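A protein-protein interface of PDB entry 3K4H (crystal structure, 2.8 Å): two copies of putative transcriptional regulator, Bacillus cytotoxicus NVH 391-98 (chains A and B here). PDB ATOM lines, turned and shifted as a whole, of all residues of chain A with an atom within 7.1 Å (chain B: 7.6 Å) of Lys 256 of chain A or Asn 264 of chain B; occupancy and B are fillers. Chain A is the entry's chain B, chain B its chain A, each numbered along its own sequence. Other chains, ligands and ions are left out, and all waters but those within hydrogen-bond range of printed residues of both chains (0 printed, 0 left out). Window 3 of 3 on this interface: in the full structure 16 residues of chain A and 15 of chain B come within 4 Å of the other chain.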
ATOM      1  N   LEU A  11      -8.098   8.071   4.810  1.00  0.00           N
ATOM      2  CA  LEU A  11      -8.986   8.669   3.817  1.00  0.00           C
ATOM      3  C   LEU A  11      -9.296   7.764   2.668  1.00  0.00           C
ATOM      4  O   LEU A  11      -8.518   6.955   2.317  1.00  0.00           O
ATOM      5  CB  LEU A  11      -8.363   9.888   3.200  1.00  0.00           C
ATOM      6  CG  LEU A  11      -7.814  10.933   4.107  1.00  0.00           C
ATOM      7  CD1 LEU A  11      -7.443  12.078   3.335  1.00  0.00           C
ATOM      8  CD2 LEU A  11      -8.874  11.285   4.985  1.00  0.00           C
ATOM      9  N   GLY A  34      -0.345  14.665  -4.675  1.00  0.00           N
ATOM     10  CA  GLY A  34      -0.769  15.775  -3.816  1.00  0.00           C
ATOM     11  C   GLY A  34      -1.497  15.267  -2.598  1.00  0.00           C
ATOM     12  O   GLY A  34      -1.190  15.652  -1.472  1.00  0.00           O
ATOM     13  N   ILE A  35      -2.434  14.353  -2.822  1.00  0.00           N
ATOM     14  CA  ILE A  35      -3.254  13.818  -1.754  1.00  0.00           C
ATOM     15  C   ILE A  35      -2.384  13.131  -0.722  1.00  0.00           C
ATOM     16  O   ILE A  35      -2.552  13.367   0.464  1.00  0.00           O
ATOM     17  CB  ILE A  35      -4.307  12.863  -2.294  1.00  0.00           C
ATOM     18  CG1 ILE A  35      -5.319  13.625  -3.176  1.00  0.00           C
ATOM     19  CG2 ILE A  35      -4.997  12.153  -1.141  1.00  0.00           C
ATOM     20  CD1 ILE A  35      -6.355  12.743  -3.862  1.00  0.00           C
ATOM     21  N   PHE A  38      -0.017  15.780   1.314  1.00  0.00           N
ATOM     22  CA  PHE A  38      -0.654  16.430   2.467  1.00  0.00           C
ATOM     23  C   PHE A  38      -1.087  15.423   3.523  1.00  0.00           C
ATOM     24  O   PHE A  38      -0.885  15.654   4.715  1.00  0.00           O
ATOM     25  CB  PHE A  38      -1.864  17.289   2.105  1.00  0.00           C
ATOM     26  CG  PHE A  38      -2.531  17.867   3.311  1.00  0.00           C
ATOM     27  CD1 PHE A  38      -2.135  19.106   3.801  1.00  0.00           C
ATOM     28  CD2 PHE A  38      -3.504  17.139   4.005  1.00  0.00           C
ATOM     29  CE1 PHE A  38      -2.717  19.627   4.940  1.00  0.00           C
ATOM     30  CE2 PHE A  38      -4.107  17.648   5.151  1.00  0.00           C
ATOM     31  CZ  PHE A  38      -3.717  18.895   5.623  1.00  0.00           C
ATOM     32  N   ALA A  39      -1.709  14.330   3.090  1.00  0.00           N
ATOM     33  CA  ALA A  39      -2.147  13.284   4.009  1.00  0.00           C
ATOM     34  C   ALA A  39      -1.057  12.926   5.031  1.00  0.00           C
ATOM     35  O   ALA A  39      -1.339  12.618   6.199  1.00  0.00           O
ATOM     36  CB  ALA A  39      -2.559  12.062   3.232  1.00  0.00           C
ATOM     37  N   VAL A  41       1.203  14.819   6.359  1.00  0.00           N
ATOM     38  CA  VAL A  41       1.352  15.868   7.362  1.00  0.00           C
ATOM     39  C   VAL A  41       0.482  15.576   8.572  1.00  0.00           C
ATOM     40  O   VAL A  41       0.874  15.842   9.701  1.00  0.00           O
ATOM     41  CB  VAL A  41       1.001  17.241   6.777  1.00  0.00           C
ATOM     42  CG1 VAL A  41       0.688  18.284   7.890  1.00  0.00           C
ATOM     43  CG2 VAL A  41       2.121  17.717   5.820  1.00  0.00           C
ATOM     44  N   GLU A  42      -0.690  15.003   8.348  1.00  0.00           N
ATOM     45  CA  GLU A  42      -1.557  14.680   9.460  1.00  0.00           C
ATOM     46  C   GLU A  42      -1.585  13.179   9.769  1.00  0.00           C
ATOM     47  O   GLU A  42      -2.375  12.730  10.588  1.00  0.00           O
ATOM     48  CB  GLU A  42      -2.956  15.230   9.193  1.00  0.00           C
ATOM     49  CG  GLU A  42      -3.000  16.745   9.095  1.00  0.00           C
ATOM     50  CD  GLU A  42      -2.471  17.437  10.353  1.00  0.00           C
ATOM     51  OE1 GLU A  42      -2.685  16.912  11.473  1.00  0.00           O
ATOM     52  OE2 GLU A  42      -1.839  18.506  10.226  1.00  0.00           O
ATOM     53  N   ILE A  74     -12.548  11.200  -0.858  1.00  0.00           N
ATOM     54  CA  ILE A  74     -12.254  12.143  -1.922  1.00  0.00           C
ATOM     55  C   ILE A  74     -12.802  11.528  -3.171  1.00  0.00           C
ATOM     56  O   ILE A  74     -12.581  10.354  -3.404  1.00  0.00           O
ATOM     57  CB  ILE A  74     -10.734  12.362  -2.107  1.00  0.00           C
ATOM     58  CG1 ILE A  74     -10.160  13.256  -1.005  1.00  0.00           C
ATOM     59  CG2 ILE A  74     -10.467  13.053  -3.410  1.00  0.00           C
ATOM     60  CD1 ILE A  74      -8.670  13.208  -0.899  1.00  0.00           C
ATOM     61  N   VAL A  96     -14.902  15.391  -0.264  1.00  0.00           N
ATOM     62  CA  VAL A  96     -14.440  16.529  -1.060  1.00  0.00           C
ATOM     63  C   VAL A  96     -14.367  16.048  -2.506  1.00  0.00           C
ATOM     64  O   VAL A  96     -14.252  14.853  -2.763  1.00  0.00           O
ATOM     65  CB  VAL A  96     -13.067  17.074  -0.524  1.00  0.00           C
ATOM     66  CG1 VAL A  96     -12.383  17.997  -1.514  1.00  0.00           C
ATOM     67  CG2 VAL A  96     -13.260  17.815   0.770  1.00  0.00           C
ATOM     68  N   LEU A 250      -3.917  20.548  -6.637  1.00  0.00           N
ATOM     69  CA  LEU A 250      -5.347  20.186  -6.541  1.00  0.00           C
ATOM     70  C   LEU A 250      -5.492  19.063  -5.521  1.00  0.00           C
ATOM     71  O   LEU A 250      -6.237  19.172  -4.552  1.00  0.00           O
ATOM     72  CB  LEU A 250      -5.977  19.745  -7.877  1.00  0.00           C
ATOM     73  CG  LEU A 250      -6.530  20.639  -9.005  1.00  0.00           C
ATOM     74  CD1 LEU A 250      -6.946  19.789 -10.208  1.00  0.00           C
ATOM     75  CD2 LEU A 250      -7.708  21.468  -8.599  1.00  0.00           C
ATOM     76  N   GLY A 251      -4.754  17.983  -5.743  1.00  0.00           N
ATOM     77  CA  GLY A 251      -4.723  16.872  -4.804  1.00  0.00           C
ATOM     78  C   GLY A 251      -4.427  17.299  -3.381  1.00  0.00           C
ATOM     79  O   GLY A 251      -5.138  16.928  -2.472  1.00  0.00           O
ATOM     80  N   TYR A 252      -3.388  18.095  -3.201  1.00  0.00           N
ATOM     81  CA  TYR A 252      -2.967  18.573  -1.874  1.00  0.00           C
ATOM     82  C   TYR A 252      -4.058  19.368  -1.188  1.00  0.00           C
ATOM     83  O   TYR A 252      -4.365  19.156  -0.016  1.00  0.00           O
ATOM     84  CB  TYR A 252      -1.735  19.467  -2.031  1.00  0.00           C
ATOM     85  CG  TYR A 252      -1.048  19.819  -0.738  1.00  0.00           C
ATOM     86  CD1 TYR A 252       0.049  19.098  -0.296  1.00  0.00           C
ATOM     87  CD2 TYR A 252      -1.474  20.900   0.029  1.00  0.00           C
ATOM     88  CE1 TYR A 252       0.687  19.434   0.888  1.00  0.00           C
ATOM     89  CE2 TYR A 252      -0.855  21.223   1.216  1.00  0.00           C
ATOM     90  CZ  TYR A 252       0.220  20.494   1.637  1.00  0.00           C
ATOM     91  OH  TYR A 252       0.849  20.838   2.814  1.00  0.00           O
ATOM     92  N   GLU A 253      -4.631  20.297  -1.944  1.00  0.00           N
ATOM     93  CA  GLU A 253      -5.635  21.195  -1.399  1.00  0.00           C
ATOM     94  C   GLU A 253      -6.968  20.479  -1.139  1.00  0.00           C
ATOM     95  O   GLU A 253      -7.675  20.792  -0.192  1.00  0.00           O
ATOM     96  CB  GLU A 253      -5.770  22.452  -2.256  1.00  0.00           C
ATOM     97  CG  GLU A 253      -5.812  23.687  -1.406  1.00  0.00           C
ATOM     98  CD  GLU A 253      -4.494  23.950  -0.722  1.00  0.00           C
ATOM     99  OE1 GLU A 253      -3.466  23.938  -1.423  1.00  0.00           O
ATOM    100  OE2 GLU A 253      -4.472  24.193   0.501  1.00  0.00           O
ATOM    101  N   ALA A 254      -7.270  19.484  -1.951  1.00  0.00           N
ATOM    102  CA  ALA A 254      -8.400  18.610  -1.705  1.00  0.00           C
ATOM    103  C   ALA A 254      -8.259  17.877  -0.380  1.00  0.00           C
ATOM    104  O   ALA A 254      -9.213  17.831   0.397  1.00  0.00           O
ATOM    105  CB  ALA A 254      -8.553  17.635  -2.833  1.00  0.00           C
ATOM    106  N   ALA A 255      -7.083  17.306  -0.114  1.00  0.00           N
ATOM    107  CA  ALA A 255      -6.868  16.575   1.149  1.00  0.00           C
ATOM    108  C   ALA A 255      -6.972  17.503   2.364  1.00  0.00           C
ATOM    109  O   ALA A 255      -7.593  17.138   3.381  1.00  0.00           O
ATOM    110  CB  ALA A 255      -5.540  15.889   1.146  1.00  0.00           C
ATOM    111  N   LYS A 256      -6.362  18.691   2.247  1.00  0.00           N
ATOM    112  CA  LYS A 256      -6.349  19.649   3.331  1.00  0.00           C
ATOM    113  C   LYS A 256      -7.785  19.934   3.695  1.00  0.00           C
ATOM    114  O   LYS A 256      -8.157  19.861   4.876  1.00  0.00           O
ATOM    115  CB  LYS A 256      -5.620  20.945   2.957  1.00  0.00           C
ATOM    116  CG  LYS A 256      -5.459  21.910   4.162  1.00  0.00           C
ATOM    117  CD  LYS A 256      -4.695  23.191   3.820  1.00  0.00           C
ATOM    118  CE  LYS A 256      -3.220  23.170   4.274  1.00  0.00           C
ATOM    119  NZ  LYS A 256      -2.988  23.507   5.735  1.00  0.00           N
ATOM    120  N   ALA A 257      -8.592  20.208   2.664  1.00  0.00           N
ATOM    121  CA  ALA A 257     -10.012  20.479   2.825  1.00  0.00           C
ATOM    122  C   ALA A 257     -10.739  19.351   3.538  1.00  0.00           C
ATOM    123  O   ALA A 257     -11.395  19.588   4.541  1.00  0.00           O
ATOM    124  CB  ALA A 257     -10.652  20.775   1.503  1.00  0.00           C
ATOM    125  N   LEU A 258     -10.599  18.122   3.059  1.00  0.00           N
ATOM    126  CA  LEU A 258     -11.279  16.983   3.682  1.00  0.00           C
ATOM    127  C   LEU A 258     -10.861  16.766   5.132  1.00  0.00           C
ATOM    128  O   LEU A 258     -11.708  16.579   6.002  1.00  0.00           O
ATOM    129  CB  LEU A 258     -11.033  15.715   2.878  1.00  0.00           C
ATOM    130  CG  LEU A 258     -11.804  14.468   3.288  1.00  0.00           C
ATOM    131  CD1 LEU A 258     -13.275  14.666   3.074  1.00  0.00           C
ATOM    132  CD2 LEU A 258     -11.332  13.298   2.477  1.00  0.00           C
ATOM    133  N   VAL A 259      -9.558  16.783   5.393  1.00  0.00           N
ATOM    134  CA  VAL A 259      -9.079  16.572   6.749  1.00  0.00           C
ATOM    135  C   VAL A 259      -9.708  17.612   7.679  1.00  0.00           C
ATOM    136  O   VAL A 259     -10.042  17.306   8.812  1.00  0.00           O
ATOM    137  CB  VAL A 259      -7.512  16.577   6.827  1.00  0.00           C
ATOM    138  CG1 VAL A 259      -7.001  16.577   8.287  1.00  0.00           C
ATOM    139  CG2 VAL A 259      -6.928  15.377   6.041  1.00  0.00           C
ATOM    140  N   ASP A 260      -9.892  18.835   7.186  1.00  0.00           N
ATOM    141  CA  ASP A 260     -10.542  19.877   7.982  1.00  0.00           C
ATOM    142  C   ASP A 260     -11.985  19.461   8.212  1.00  0.00           C
ATOM    143  O   ASP A 260     -12.444  19.418   9.339  1.00  0.00           O
ATOM    144  CB  ASP A 260     -10.430  21.240   7.295  1.00  0.00           C
ATOM    145  CG  ASP A 260     -11.247  22.332   7.979  1.00  0.00           C
ATOM    146  OD1 ASP A 260     -11.149  22.484   9.212  1.00  0.00           O
ATOM    147  OD2 ASP A 260     -11.975  23.062   7.266  1.00  0.00           O
ATOM    148  N   LYS A 261     -12.675  19.097   7.140  1.00  0.00           N
ATOM    149  CA  LYS A 261     -14.039  18.593   7.225  1.00  0.00           C
ATOM    150  C   LYS A 261     -14.169  17.439   8.237  1.00  0.00           C
ATOM    151  O   LYS A 261     -15.114  17.391   9.013  1.00  0.00           O
ATOM    152  CB  LYS A 261     -14.486  18.147   5.836  1.00  0.00           C
ATOM    153  CG  LYS A 261     -15.902  18.484   5.454  1.00  0.00           C
ATOM    154  CD  LYS A 261     -15.926  18.983   4.011  1.00  0.00           C
ATOM    155  CE  LYS A 261     -17.211  18.651   3.314  1.00  0.00           C
ATOM    156  NZ  LYS A 261     -18.227  19.698   3.579  1.00  0.00           N
ATOM    157  N   VAL A 262     -13.203  16.534   8.248  1.00  0.00           N
ATOM    158  CA  VAL A 262     -13.295  15.332   9.062  1.00  0.00           C
ATOM    159  C   VAL A 262     -13.115  15.643  10.544  1.00  0.00           C
ATOM    160  O   VAL A 262     -13.771  15.047  11.396  1.00  0.00           O
ATOM    161  CB  VAL A 262     -12.270  14.246   8.575  1.00  0.00           C
ATOM    162  CG1 VAL A 262     -12.044  13.142   9.625  1.00  0.00           C
ATOM    163  CG2 VAL A 262     -12.731  13.631   7.251  1.00  0.00           C
ATOM    164  N   ILE A 272     -12.366  25.704  -3.654  1.00  0.00           N
ATOM    165  CA  ILE A 272     -10.975  26.098  -3.523  1.00  0.00           C
ATOM    166  C   ILE A 272     -10.398  26.093  -4.914  1.00  0.00           C
ATOM    167  O   ILE A 272     -10.576  25.122  -5.638  1.00  0.00           O
ATOM    168  CB  ILE A 272     -10.207  25.130  -2.594  1.00  0.00           C
ATOM    169  CG1 ILE A 272     -11.037  24.869  -1.335  1.00  0.00           C
ATOM    170  CG2 ILE A 272      -8.850  25.701  -2.229  1.00  0.00           C
ATOM    171  CD1 ILE A 272     -10.728  23.577  -0.653  1.00  0.00           C
ATOM    172  N   LEU B 258      -6.230  32.829   7.366  1.00  0.00           N
ATOM    173  CA  LEU B 258      -5.126  33.610   7.922  1.00  0.00           C
ATOM    174  C   LEU B 258      -4.452  32.881   9.072  1.00  0.00           C
ATOM    175  O   LEU B 258      -3.233  32.815   9.127  1.00  0.00           O
ATOM    176  CB  LEU B 258      -5.596  34.988   8.377  1.00  0.00           C
ATOM    177  CG  LEU B 258      -4.548  35.855   9.071  1.00  0.00           C
ATOM    178  CD1 LEU B 258      -3.317  36.103   8.177  1.00  0.00           C
ATOM    179  CD2 LEU B 258      -5.141  37.167   9.575  1.00  0.00           C
ATOM    180  N   VAL B 259      -5.252  32.336   9.982  1.00  0.00           N
ATOM    181  CA  VAL B 259      -4.726  31.651  11.152  1.00  0.00           C
ATOM    182  C   VAL B 259      -3.932  30.439  10.695  1.00  0.00           C
ATOM    183  O   VAL B 259      -2.872  30.131  11.235  1.00  0.00           O
ATOM    184  CB  VAL B 259      -5.863  31.266  12.137  1.00  0.00           C
ATOM    185  CG1 VAL B 259      -5.407  30.286  13.187  1.00  0.00           C
ATOM    186  CG2 VAL B 259      -6.381  32.511  12.824  1.00  0.00           C
ATOM    187  N   ASP B 260      -4.429  29.767   9.668  1.00  0.00           N
ATOM    188  CA  ASP B 260      -3.717  28.627   9.111  1.00  0.00           C
ATOM    189  C   ASP B 260      -2.354  29.123   8.621  1.00  0.00           C
ATOM    190  O   ASP B 260      -1.316  28.601   9.003  1.00  0.00           O
ATOM    191  CB  ASP B 260      -4.538  27.991   7.993  1.00  0.00           C
ATOM    192  CG  ASP B 260      -3.836  26.839   7.336  1.00  0.00           C
ATOM    193  OD1 ASP B 260      -3.440  25.861   8.023  1.00  0.00           O
ATOM    194  OD2 ASP B 260      -3.684  26.911   6.106  1.00  0.00           O
ATOM    195  N   LYS B 261      -2.375  30.184   7.828  1.00  0.00           N
ATOM    196  CA  LYS B 261      -1.160  30.813   7.324  1.00  0.00           C
ATOM    197  C   LYS B 261      -0.220  31.207   8.451  1.00  0.00           C
ATOM    198  O   LYS B 261       0.989  31.049   8.323  1.00  0.00           O
ATOM    199  CB  LYS B 261      -1.526  32.040   6.505  1.00  0.00           C
ATOM    200  CG  LYS B 261      -0.378  32.652   5.733  1.00  0.00           C
ATOM    201  CD  LYS B 261      -0.900  33.427   4.513  1.00  0.00           C
ATOM    202  CE  LYS B 261       0.246  34.054   3.765  1.00  0.00           C
ATOM    203  NZ  LYS B 261       0.045  33.911   2.311  1.00  0.00           N
ATOM    204  N   VAL B 262      -0.782  31.744   9.505  1.00  0.00           N
ATOM    205  CA  VAL B 262       0.036  32.129  10.604  1.00  0.00           C
ATOM    206  C   VAL B 262       0.546  30.998  11.397  1.00  0.00           C
ATOM    207  O   VAL B 262       1.703  30.926  11.684  1.00  0.00           O
ATOM    208  CB  VAL B 262      -0.765  32.930  11.553  1.00  0.00           C
ATOM    209  CG1 VAL B 262      -0.063  33.063  12.772  1.00  0.00           C
ATOM    210  CG2 VAL B 262      -1.001  34.231  11.010  1.00  0.00           C
ATOM    211  N   GLU B 263      -0.323  30.142  11.862  1.00  0.00           N
ATOM    212  CA  GLU B 263       0.209  29.009  12.536  1.00  0.00           C
ATOM    213  C   GLU B 263       1.027  27.974  11.810  1.00  0.00           C
ATOM    214  O   GLU B 263       2.022  27.534  12.313  1.00  0.00           O
ATOM    215  CB  GLU B 263      -0.885  28.376  13.336  1.00  0.00           C
ATOM    216  CG  GLU B 263      -1.419  29.347  14.281  1.00  0.00           C
ATOM    217  CD  GLU B 263      -2.470  28.796  15.089  1.00  0.00           C
ATOM    218  OE1 GLU B 263      -2.844  27.664  14.847  1.00  0.00           O
ATOM    219  OE2 GLU B 263      -2.944  29.493  15.963  1.00  0.00           O
ATOM    220  N   ASN B 264       0.622  27.550  10.633  1.00  0.00           N
ATOM    221  CA  ASN B 264       1.472  26.613   9.948  1.00  0.00           C
ATOM    222  C   ASN B 264       2.813  27.072   9.491  1.00  0.00           C
ATOM    223  O   ASN B 264       3.796  26.374   9.530  1.00  0.00           O
ATOM    224  CB  ASN B 264       0.716  25.757   8.979  1.00  0.00           C
ATOM    225  CG  ASN B 264      -0.224  24.847   9.692  1.00  0.00           C
ATOM    226  OD1 ASN B 264      -0.411  24.977  10.883  1.00  0.00           O
ATOM    227  ND2 ASN B 264      -0.809  23.916   8.985  1.00  0.00           N
ATOM    228  N   ALA B 265       2.817  28.251   8.956  1.00  0.00           N
ATOM    229  CA  ALA B 265       3.923  29.131   8.852  1.00  0.00           C
ATOM    230  C   ALA B 265       4.727  28.668   7.697  1.00  0.00           C
ATOM    231  O   ALA B 265       5.688  29.294   7.332  1.00  0.00           O
ATOM    232  CB  ALA B 265       4.750  29.113  10.106  1.00  0.00           C
ATOM    233  N   GLU B 266       4.305  27.609   7.049  1.00  0.00           N
ATOM    234  CA  GLU B 266       4.931  27.286   5.807  1.00  0.00           C
ATOM    235  C   GLU B 266       3.683  27.253   5.057  1.00  0.00           C
ATOM    236  O   GLU B 266       2.757  26.590   5.479  1.00  0.00           O
ATOM    237  CB  GLU B 266       5.539  25.922   5.883  1.00  0.00           C
ATOM    238  CG  GLU B 266       6.720  25.880   6.777  1.00  0.00           C
ATOM    239  CD  GLU B 266       7.829  25.061   6.205  1.00  0.00           C
ATOM    240  OE1 GLU B 266       7.675  23.838   6.125  1.00  0.00           O
ATOM    241  OE2 GLU B 266       8.861  25.635   5.831  1.00  0.00           O
ATOM    242  N   SER B 267       3.584  27.951   3.963  1.00  0.00           N
ATOM    243  CA  SER B 267       2.279  27.930   3.393  1.00  0.00           C
ATOM    244  C   SER B 267       2.189  28.010   1.926  1.00  0.00           C
ATOM    245  O   SER B 267       3.089  28.468   1.261  1.00  0.00           O
ATOM    246  CB  SER B 267       1.343  28.882   4.117  1.00  0.00           C
ATOM    247  OG  SER B 267       0.929  28.276   5.327  1.00  0.00           O
ATOM    248  N   THR B 268       1.075  27.543   1.430  1.00  0.00           N
ATOM    249  CA  THR B 268       0.806  27.650   0.041  1.00  0.00           C
ATOM    250  C   THR B 268      -0.340  28.601  -0.100  1.00  0.00           C
ATOM    251  O   THR B 268      -1.244  28.618   0.705  1.00  0.00           O
ATOM    252  CB  THR B 268       0.392  26.340  -0.512  1.00  0.00           C
ATOM    253  OG1 THR B 268       0.594  25.328   0.483  1.00  0.00           O
ATOM    254  CG2 THR B 268       1.203  26.058  -1.723  1.00  0.00           C
ATOM    255  N   LYS B 270      -3.563  29.863  -1.844  1.00  0.00           N
ATOM    256  CA  LYS B 270      -4.766  29.424  -2.527  1.00  0.00           C
ATOM    257  C   LYS B 270      -5.757  30.573  -2.578  1.00  0.00           C
ATOM    258  O   LYS B 270      -5.572  31.592  -1.924  1.00  0.00           O
ATOM    259  CB  LYS B 270      -5.402  28.274  -1.749  1.00  0.00           C
ATOM    260  CG  LYS B 270      -5.548  28.587  -0.268  1.00  0.00           C
ATOM    261  CD  LYS B 270      -6.068  27.415   0.508  1.00  0.00           C
ATOM    262  CE  LYS B 270      -5.169  27.146   1.710  1.00  0.00           C
ATOM    263  NZ  LYS B 270      -5.943  27.201   3.000  1.00  0.00           N
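OD1 of Asp 260 of chain B lies within hydrogen-bond range of ND2 of Asn 264 of chain B (3.4 Å). OD2 of Asp 260 of chain B is in salt-bridge range of NZ of Lys 270 of chain B, 3.9 Å away.
Of the 23 printed residues of chain A, 2 touch a printed residue of chain B. Of the 12 printed residues of chain B, 3 touch a printed residue of chain A. Among the printed residues, 3 pairs touch across the chains.
OD1 of Asp 260 of chain B is in salt-bridge range of NZ of Lys 256 of chain A (3.3 Å).
Lys 256 of chain A touches two residues of chain B. Asn 264 of chain B touches just one residue of chain A: Lys 256 (3.9 Å). Ala 255 of chain A touches none of the printed residues of chain B. Of the printed residues of chain A, Lys 270 of chain B touches Glu 253. Of the printed residues of chain A, Asp 260 of chain B touches Lys 256. Of the printed residues of chain B, Glu 253 of chain A touches Lys 270 (3.3 Å). Gly 251 of chain A touches none of the printed residues of chain B. The nearest residue of chain B that does not touch Lys 256 of chain A is Lys 270 of chain B (4.3 Å). The nearest residue of chain A that does not touch Asn 264 of chain B is Glu 42 of chain A (5.6 Å).
Positions printed for both chains: 258, 259, 260, 261 and 262. Of the 3 pairs that touch across the chains among the printed residues, none has its exchanged pair printed and touching as well.
Among the printed residues, pairs that only touch across the chains: Glu 253 of chain A with Lys 270 of chain B (3.3 Å) and Lys 256 of chain A with Asn 264 of chain B (3.9 Å).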
